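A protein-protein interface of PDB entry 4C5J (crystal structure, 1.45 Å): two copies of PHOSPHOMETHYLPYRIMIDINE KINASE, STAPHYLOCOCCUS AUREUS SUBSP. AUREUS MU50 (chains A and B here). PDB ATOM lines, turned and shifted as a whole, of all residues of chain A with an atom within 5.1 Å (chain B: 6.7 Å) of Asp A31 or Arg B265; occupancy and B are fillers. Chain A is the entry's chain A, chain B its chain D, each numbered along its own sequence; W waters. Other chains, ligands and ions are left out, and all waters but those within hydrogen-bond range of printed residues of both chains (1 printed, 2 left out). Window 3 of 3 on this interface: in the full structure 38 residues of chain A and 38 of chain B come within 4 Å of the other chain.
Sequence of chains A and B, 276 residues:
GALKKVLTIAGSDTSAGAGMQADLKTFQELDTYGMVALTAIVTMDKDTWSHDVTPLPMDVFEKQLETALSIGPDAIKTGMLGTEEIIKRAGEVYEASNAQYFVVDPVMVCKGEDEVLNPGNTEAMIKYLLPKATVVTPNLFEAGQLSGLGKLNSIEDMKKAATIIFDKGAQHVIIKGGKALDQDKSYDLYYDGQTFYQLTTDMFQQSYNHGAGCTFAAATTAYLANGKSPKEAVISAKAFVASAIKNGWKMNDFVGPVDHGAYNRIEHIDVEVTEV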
ATOM      1  N   LEU A   3      21.566  34.046 -15.052  1.00  0.00           N
ATOM      2  CA  LEU A   3      20.305  33.830 -15.727  1.00  0.00           C
ATOM      3  C   LEU A   3      19.340  34.984 -15.333  1.00  0.00           C
ATOM      4  O   LEU A   3      19.235  35.393 -14.164  1.00  0.00           O
ATOM      5  CB  LEU A   3      19.683  32.522 -15.292  1.00  0.00           C
ATOM      6  CG  LEU A   3      20.347  31.256 -15.661  1.00  0.00           C
ATOM      7  CD1 LEU A   3      19.745  30.087 -14.979  1.00  0.00           C
ATOM      8  CD2 LEU A   3      20.251  31.082 -17.168  1.00  0.00           C
ATOM      9  N   LYS A   4      18.657  35.496 -16.341  1.00  0.00           N
ATOM     10  CA  LYS A   4      17.618  36.485 -16.099  1.00  0.00           C
ATOM     11  C   LYS A   4      16.394  35.835 -15.467  1.00  0.00           C
ATOM     12  O   LYS A   4      15.991  34.745 -15.938  1.00  0.00           O
ATOM     13  CB  LYS A   4      17.238  37.172 -17.381  1.00  0.00           C
ATOM     14  CG  LYS A   4      18.391  37.979 -18.014  1.00  0.00           C
ATOM     15  CD  LYS A   4      18.813  39.172 -17.228  1.00  0.00           C
ATOM     16  CE  LYS A   4      19.968  39.912 -17.874  1.00  0.00           C
ATOM     17  NZ  LYS A   4      20.374  41.011 -16.995  1.00  0.00           N
ATOM     18  N   PHE A  27      10.434  29.988 -21.424  1.00  0.00           N
ATOM     19  CA  PHE A  27      11.480  30.580 -20.622  1.00  0.00           C
ATOM     20  C   PHE A  27      12.726  29.693 -20.575  1.00  0.00           C
ATOM     21  O   PHE A  27      13.850  30.136 -20.710  1.00  0.00           O
ATOM     22  CB  PHE A  27      11.034  30.993 -19.219  1.00  0.00           C
ATOM     23  CG  PHE A  27       9.906  31.969 -19.147  1.00  0.00           C
ATOM     24  CD1 PHE A  27       9.581  32.839 -20.226  1.00  0.00           C
ATOM     25  CD2 PHE A  27       9.166  32.024 -17.997  1.00  0.00           C
ATOM     26  CE1 PHE A  27       8.556  33.748 -20.060  1.00  0.00           C
ATOM     27  CE2 PHE A  27       8.146  32.927 -17.873  1.00  0.00           C
ATOM     28  CZ  PHE A  27       7.876  33.809 -18.897  1.00  0.00           C
ATOM     29  N   GLN A  28      12.498  28.375 -20.450  1.00  0.00           N
ATOM     30  CA  GLN A  28      13.573  27.429 -20.276  1.00  0.00           C
ATOM     31  C   GLN A  28      14.312  27.289 -21.609  1.00  0.00           C
ATOM     32  O   GLN A  28      15.553  27.276 -21.668  1.00  0.00           O
ATOM     33  CB  GLN A  28      13.085  26.090 -19.800  1.00  0.00           C
ATOM     34  CG  GLN A  28      14.204  25.158 -19.382  1.00  0.00           C
ATOM     35  CD  GLN A  28      14.915  25.651 -18.148  1.00  0.00           C
ATOM     36  OE1 GLN A  28      14.371  26.385 -17.340  1.00  0.00           O
ATOM     37  NE2 GLN A  28      16.171  25.310 -18.061  1.00  0.00           N
ATOM     38  N   GLU A  29      13.566  27.206 -22.722  1.00  0.00           N
ATOM     39  CA  GLU A  29      14.130  27.111 -24.071  1.00  0.00           C
ATOM     40  C   GLU A  29      14.965  28.313 -24.435  1.00  0.00           C
ATOM     41  O   GLU A  29      15.922  28.214 -25.209  1.00  0.00           O
ATOM     42  CB  GLU A  29      12.948  27.028 -25.085  1.00  0.00           C
ATOM     43  CG  GLU A  29      12.258  25.683 -25.158  1.00  0.00           C
ATOM     44  CD  GLU A  29      13.126  24.524 -25.650  1.00  0.00           C
ATOM     45  OE1 GLU A  29      14.092  24.765 -26.445  1.00  0.00           O
ATOM     46  OE2 GLU A  29      12.794  23.389 -25.343  1.00  0.00           O
ATOM     47  N   LEU A  30      14.665  29.432 -23.826  1.00  0.00           N
ATOM     48  CA  LEU A  30      15.354  30.688 -24.101  1.00  0.00           C
ATOM     49  C   LEU A  30      16.377  31.042 -23.037  1.00  0.00           C
ATOM     50  O   LEU A  30      16.805  32.217 -22.918  1.00  0.00           O
ATOM     51  CB  LEU A  30      14.358  31.808 -24.403  1.00  0.00           C
ATOM     52  CG  LEU A  30      13.570  31.547 -25.687  1.00  0.00           C
ATOM     53  CD1 LEU A  30      12.515  32.646 -25.854  1.00  0.00           C
ATOM     54  CD2 LEU A  30      14.452  31.501 -26.923  1.00  0.00           C
ATOM     55  N   ASP A  31      16.791  30.047 -22.241  1.00  0.00           N
ATOM     56  CA  ASP A  31      17.892  30.262 -21.335  1.00  0.00           C
ATOM     57  C   ASP A  31      17.692  31.379 -20.339  1.00  0.00           C
ATOM     58  O   ASP A  31      18.600  32.117 -20.028  1.00  0.00           O
ATOM     59  CB  ASP A  31      19.218  30.436 -22.115  1.00  0.00           C
ATOM     60  CG  ASP A  31      19.484  29.249 -22.979  1.00  0.00           C
ATOM     61  OD1 ASP A  31      19.299  28.124 -22.489  1.00  0.00           O
ATOM     62  OD2 ASP A  31      19.917  29.382 -24.158  1.00  0.00           O
ATOM     63  N   THR A  32      16.504  31.384 -19.700  1.00  0.00           N
ATOM     64  CA  THR A  32      16.156  32.256 -18.611  1.00  0.00           C
ATOM     65  C   THR A  32      15.713  31.419 -17.427  1.00  0.00           C
ATOM     66  O   THR A  32      15.436  30.231 -17.594  1.00  0.00           O
ATOM     67  CB  THR A  32      15.054  33.267 -18.988  1.00  0.00           C
ATOM     68  OG1 THR A  32      13.826  32.643 -19.257  1.00  0.00           O
ATOM     69  CG2 THR A  32      15.481  34.125 -20.230  1.00  0.00           C
ATOM     70  N   TYR A  33      15.620  32.039 -16.253  1.00  0.00           N
ATOM     71  CA  TYR A  33      15.135  31.381 -15.058  1.00  0.00           C
ATOM     72  C   TYR A  33      13.649  31.662 -14.854  1.00  0.00           C
ATOM     73  O   TYR A  33      13.269  32.767 -14.460  1.00  0.00           O
ATOM     74  CB  TYR A  33      15.885  31.908 -13.847  1.00  0.00           C
ATOM     75  CG  TYR A  33      15.536  31.164 -12.575  1.00  0.00           C
ATOM     76  CD1 TYR A  33      16.043  29.884 -12.331  1.00  0.00           C
ATOM     77  CD2 TYR A  33      14.666  31.693 -11.643  1.00  0.00           C
ATOM     78  CE1 TYR A  33      15.729  29.148 -11.186  1.00  0.00           C
ATOM     79  CE2 TYR A  33      14.340  30.982 -10.422  1.00  0.00           C
ATOM     80  CZ  TYR A  33      14.877  29.708 -10.225  1.00  0.00           C
ATOM     81  OH  TYR A  33      14.594  29.013  -9.104  1.00  0.00           O
ATOM     82  N   ASN A 226      16.814  39.112 -22.036  1.00  0.00           N
ATOM     83  CA  ASN A 226      18.159  38.753 -22.510  1.00  0.00           C
ATOM     84  C   ASN A 226      18.817  39.836 -23.400  1.00  0.00           C
ATOM     85  O   ASN A 226      19.888  39.616 -23.937  1.00  0.00           O
ATOM     86  CB  ASN A 226      18.157  37.412 -23.197  1.00  0.00           C
ATOM     87  CG  ASN A 226      18.036  36.272 -22.248  1.00  0.00           C
ATOM     88  OD1 ASN A 226      18.433  36.348 -21.116  1.00  0.00           O
ATOM     89  ND2 ASN A 226      17.607  35.121 -22.812  1.00  0.00           N
ATOM     90  N   GLU B  29      14.304  20.388 -20.985  1.00  0.00           N
ATOM     91  CA  GLU B  29      15.718  20.239 -21.345  1.00  0.00           C
ATOM     92  C   GLU B  29      15.962  18.961 -22.081  1.00  0.00           C
ATOM     93  O   GLU B  29      16.898  18.852 -22.866  1.00  0.00           O
ATOM     94  CB  GLU B  29      16.585  20.349 -20.096  1.00  0.00           C
ATOM     95  CG  GLU B  29      16.782  21.740 -19.513  1.00  0.00           C
ATOM     96  CD  GLU B  29      17.501  22.689 -20.452  1.00  0.00           C
ATOM     97  OE1 GLU B  29      18.425  22.225 -21.183  1.00  0.00           O
ATOM     98  OE2 GLU B  29      17.224  23.903 -20.417  1.00  0.00           O
ATOM     99  N   ASN B 247      26.784  24.467 -11.328  1.00  0.00           N
ATOM    100  CA  ASN B 247      26.436  25.734 -11.948  1.00  0.00           C
ATOM    101  C   ASN B 247      25.232  26.442 -11.288  1.00  0.00           C
ATOM    102  O   ASN B 247      24.688  27.392 -11.826  1.00  0.00           O
ATOM    103  CB  ASN B 247      26.235  25.482 -13.443  1.00  0.00           C
ATOM    104  CG  ASN B 247      27.550  25.191 -14.113  1.00  0.00           C
ATOM    105  OD1 ASN B 247      28.411  26.075 -14.270  1.00  0.00           O
ATOM    106  ND2 ASN B 247      27.701  23.950 -14.522  1.00  0.00           N
ATOM    107  N   ASP B 259      21.115  24.982 -11.660  1.00  0.00           N
ATOM    108  CA  ASP B 259      20.878  25.398 -13.037  1.00  0.00           C
ATOM    109  C   ASP B 259      20.439  24.255 -13.912  1.00  0.00           C
ATOM    110  O   ASP B 259      21.267  23.493 -14.360  1.00  0.00           O
ATOM    111  CB  ASP B 259      22.086  26.132 -13.606  1.00  0.00           C
ATOM    112  CG  ASP B 259      21.858  26.686 -15.004  1.00  0.00           C
ATOM    113  OD1 ASP B 259      20.851  26.341 -15.659  1.00  0.00           O
ATOM    114  OD2 ASP B 259      22.732  27.438 -15.489  1.00  0.00           O
ATOM    115  N   HIS B 260      19.131  24.062 -14.010  1.00  0.00           N
ATOM    116  CA  HIS B 260      18.572  22.900 -14.705  1.00  0.00           C
ATOM    117  C   HIS B 260      19.085  22.727 -16.117  1.00  0.00           C
ATOM    118  O   HIS B 260      19.157  21.633 -16.646  1.00  0.00           O
ATOM    119  CB  HIS B 260      17.035  22.877 -14.711  1.00  0.00           C
ATOM    120  CG  HIS B 260      16.463  23.286 -13.397  1.00  0.00           C
ATOM    121  ND1 HIS B 260      16.387  24.608 -13.030  1.00  0.00           N
ATOM    122  CD2 HIS B 260      16.051  22.561 -12.314  1.00  0.00           C
ATOM    123  CE1 HIS B 260      15.900  24.668 -11.797  1.00  0.00           C
ATOM    124  NE2 HIS B 260      15.691  23.443 -11.344  1.00  0.00           N
ATOM    125  N   GLY B 261      19.404  23.851 -16.740  1.00  0.00           N
ATOM    126  CA  GLY B 261      19.896  23.833 -18.128  1.00  0.00           C
ATOM    127  C   GLY B 261      21.408  23.669 -18.297  1.00  0.00           C
ATOM    128  O   GLY B 261      21.894  23.715 -19.431  1.00  0.00           O
ATOM    129  N   ALA B 262      22.148  23.503 -17.200  1.00  0.00           N
ATOM    130  CA  ALA B 262      23.594  23.525 -17.318  1.00  0.00           C
ATOM    131  C   ALA B 262      24.145  22.381 -18.071  1.00  0.00           C
ATOM    132  O   ALA B 262      25.156  22.539 -18.791  1.00  0.00           O
ATOM    133  CB  ALA B 262      24.225  23.512 -15.958  1.00  0.00           C
ATOM    134  N   TYR B 263      23.563  21.180 -17.969  1.00  0.00           N
ATOM    135  CA  TYR B 263      24.065  20.022 -18.711  1.00  0.00           C
ATOM    136  C   TYR B 263      24.144  20.286 -20.236  1.00  0.00           C
ATOM    137  O   TYR B 263      25.157  19.964 -20.873  1.00  0.00           O
ATOM    138  CB  TYR B 263      23.256  18.807 -18.396  1.00  0.00           C
ATOM    139  CG  TYR B 263      23.707  17.515 -19.063  1.00  0.00           C
ATOM    140  CD1 TYR B 263      24.715  16.761 -18.452  1.00  0.00           C
ATOM    141  CD2 TYR B 263      23.122  17.011 -20.166  1.00  0.00           C
ATOM    142  CE1 TYR B 263      25.131  15.530 -18.954  1.00  0.00           C
ATOM    143  CE2 TYR B 263      23.522  15.794 -20.716  1.00  0.00           C
ATOM    144  CZ  TYR B 263      24.537  15.061 -20.109  1.00  0.00           C
ATOM    145  OH  TYR B 263      24.894  13.885 -20.671  1.00  0.00           O
ATOM    146  N   ASN B 264      23.094  20.879 -20.788  1.00  0.00           N
ATOM    147  CA  ASN B 264      23.039  21.140 -22.207  1.00  0.00           C
ATOM    148  C   ASN B 264      23.756  22.443 -22.617  1.00  0.00           C
ATOM    149  O   ASN B 264      24.317  22.556 -23.703  1.00  0.00           O
ATOM    150  CB  ASN B 264      21.599  21.196 -22.648  1.00  0.00           C
ATOM    151  CG  ASN B 264      20.953  19.844 -22.689  1.00  0.00           C
ATOM    152  OD1 ASN B 264      21.617  18.824 -22.815  1.00  0.00           O
ATOM    153  ND2 ASN B 264      19.663  19.807 -22.407  1.00  0.00           N
ATOM    154  N   ARG B 265      23.751  23.429 -21.746  1.00  0.00           N
ATOM    155  CA  ARG B 265      24.232  24.767 -22.117  1.00  0.00           C
ATOM    156  C   ARG B 265      25.683  25.051 -21.727  1.00  0.00           C
ATOM    157  O   ARG B 265      26.363  25.806 -22.396  1.00  0.00           O
ATOM    158  CB  ARG B 265      23.304  25.839 -21.516  1.00  0.00           C
ATOM    159  CG  ARG B 265      23.722  27.288 -21.717  1.00  0.00           C
ATOM    160  CD  ARG B 265      22.742  28.356 -21.168  1.00  0.00           C
ATOM    161  NE  ARG B 265      21.768  27.834 -20.320  1.00  0.00           N
ATOM    162  CZ  ARG B 265      21.868  27.714 -18.989  1.00  0.00           C
ATOM    163  NH1 ARG B 265      22.882  28.198 -18.282  1.00  0.00           N
ATOM    164  NH2 ARG B 265      20.866  27.223 -18.413  1.00  0.00           N
ATOM    165  N   ILE B 266      26.135  24.453 -20.649  1.00  0.00           N
ATOM    166  CA  ILE B 266      27.399  24.758 -20.005  1.00  0.00           C
ATOM    167  C   ILE B 266      28.408  23.613 -20.143  1.00  0.00           C
ATOM    168  O   ILE B 266      29.488  23.835 -20.722  1.00  0.00           O
ATOM    169  CB  ILE B 266      27.268  25.197 -18.556  1.00  0.00           C
ATOM    170  CG1 ILE B 266      26.342  26.366 -18.441  1.00  0.00           C
ATOM    171  CG2 ILE B 266      28.664  25.496 -17.988  1.00  0.00           C
ATOM    172  CD1 ILE B 266      26.039  26.896 -17.042  1.00  0.00           C
ATOM    173  N   GLU B 267      28.102  22.443 -19.577  1.00  0.00           N
ATOM    174  CA  GLU B 267      29.041  21.313 -19.501  1.00  0.00           C
ATOM    175  C   GLU B 267      28.422  20.030 -18.991  1.00  0.00           C
ATOM    176  O   GLU B 267      27.441  20.072 -18.238  1.00  0.00           O
ATOM    177  CB  GLU B 267      30.270  21.647 -18.602  1.00  0.00           C
ATOM    178  CG  GLU B 267      29.862  21.785 -17.121  1.00  0.00           C
ATOM    179  CD  GLU B 267      30.882  22.507 -16.229  1.00  0.00           C
ATOM    180  OE1 GLU B 267      32.107  22.372 -16.436  1.00  0.00           O
ATOM    181  OE2 GLU B 267      30.475  23.264 -15.401  1.00  0.00           O
HETATM  182  O   HOH W   1      17.144  25.256 -22.801  1.00  0.00           O
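The backbone carbonyl oxygen (O) of Glu B29 is in hydrogen-bond range of the side-chain amide nitrogen (ND2) of Asn B264 (3.0 Å). The side-chain carboxylate (OD1) of Asp B259 lies close to the backbone NH (N) of Gly B261 (3.1 Å). OD1 of Asp B259 lies within hydrogen-bond range of N of Ala B262 (3.5 Å). The side-chain carboxylate of Asp B259 lies within salt-bridge range of the guanidinium group of Arg B265 (2.9 Å).
1 position is printed for both chains.
Among the printed residues, pairs that only touch across the chains: Leu A3 with Asp B259 and Gln A28 with Gly B261.
Water W1 lies within hydrogen-bond range of the side-chain carboxylate of Glu B29 (2.7 Å) and the backbone carbonyl oxygen of Gln A28 (2.8 Å).
The side-chain carboxylate (OE2) of Glu B29 lies within hydrogen-bond range of the side-chain amide nitrogen (NE2) of Gln A28, at 2.9 Å. OD1 of Asp A31 lies within salt-bridge range of NE of Arg B265 (3.3 Å).
Of the printed residues of chain B, Leu A3 touches Asp B259 (3.96 Å). Of the printed residues of chain B, Gln A28 touches Glu B29 (2.9 Å) and Gly B261 (3.8 Å). Of the printed residues of chain A, Asp B259 touches Leu A3. Of the printed residues of chain A, Gly B261 touches Gln A28 (3.8 Å). Of chain A, only Asp A31 comes within 4 Å of Arg B265. The nearest residue of chain B that does not touch Asp A31 is Glu B29 (5.1 Å). The nearest printed residue of chain B that does not touch Leu A3 is Arg B265 (4.1 Å).
Hydrophobic or aromatic side chains of chain A that line the printed part of chain B: Leu A3. Along chain A the printed residues that touch a printed residue of chain B span positions 3 to 31.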
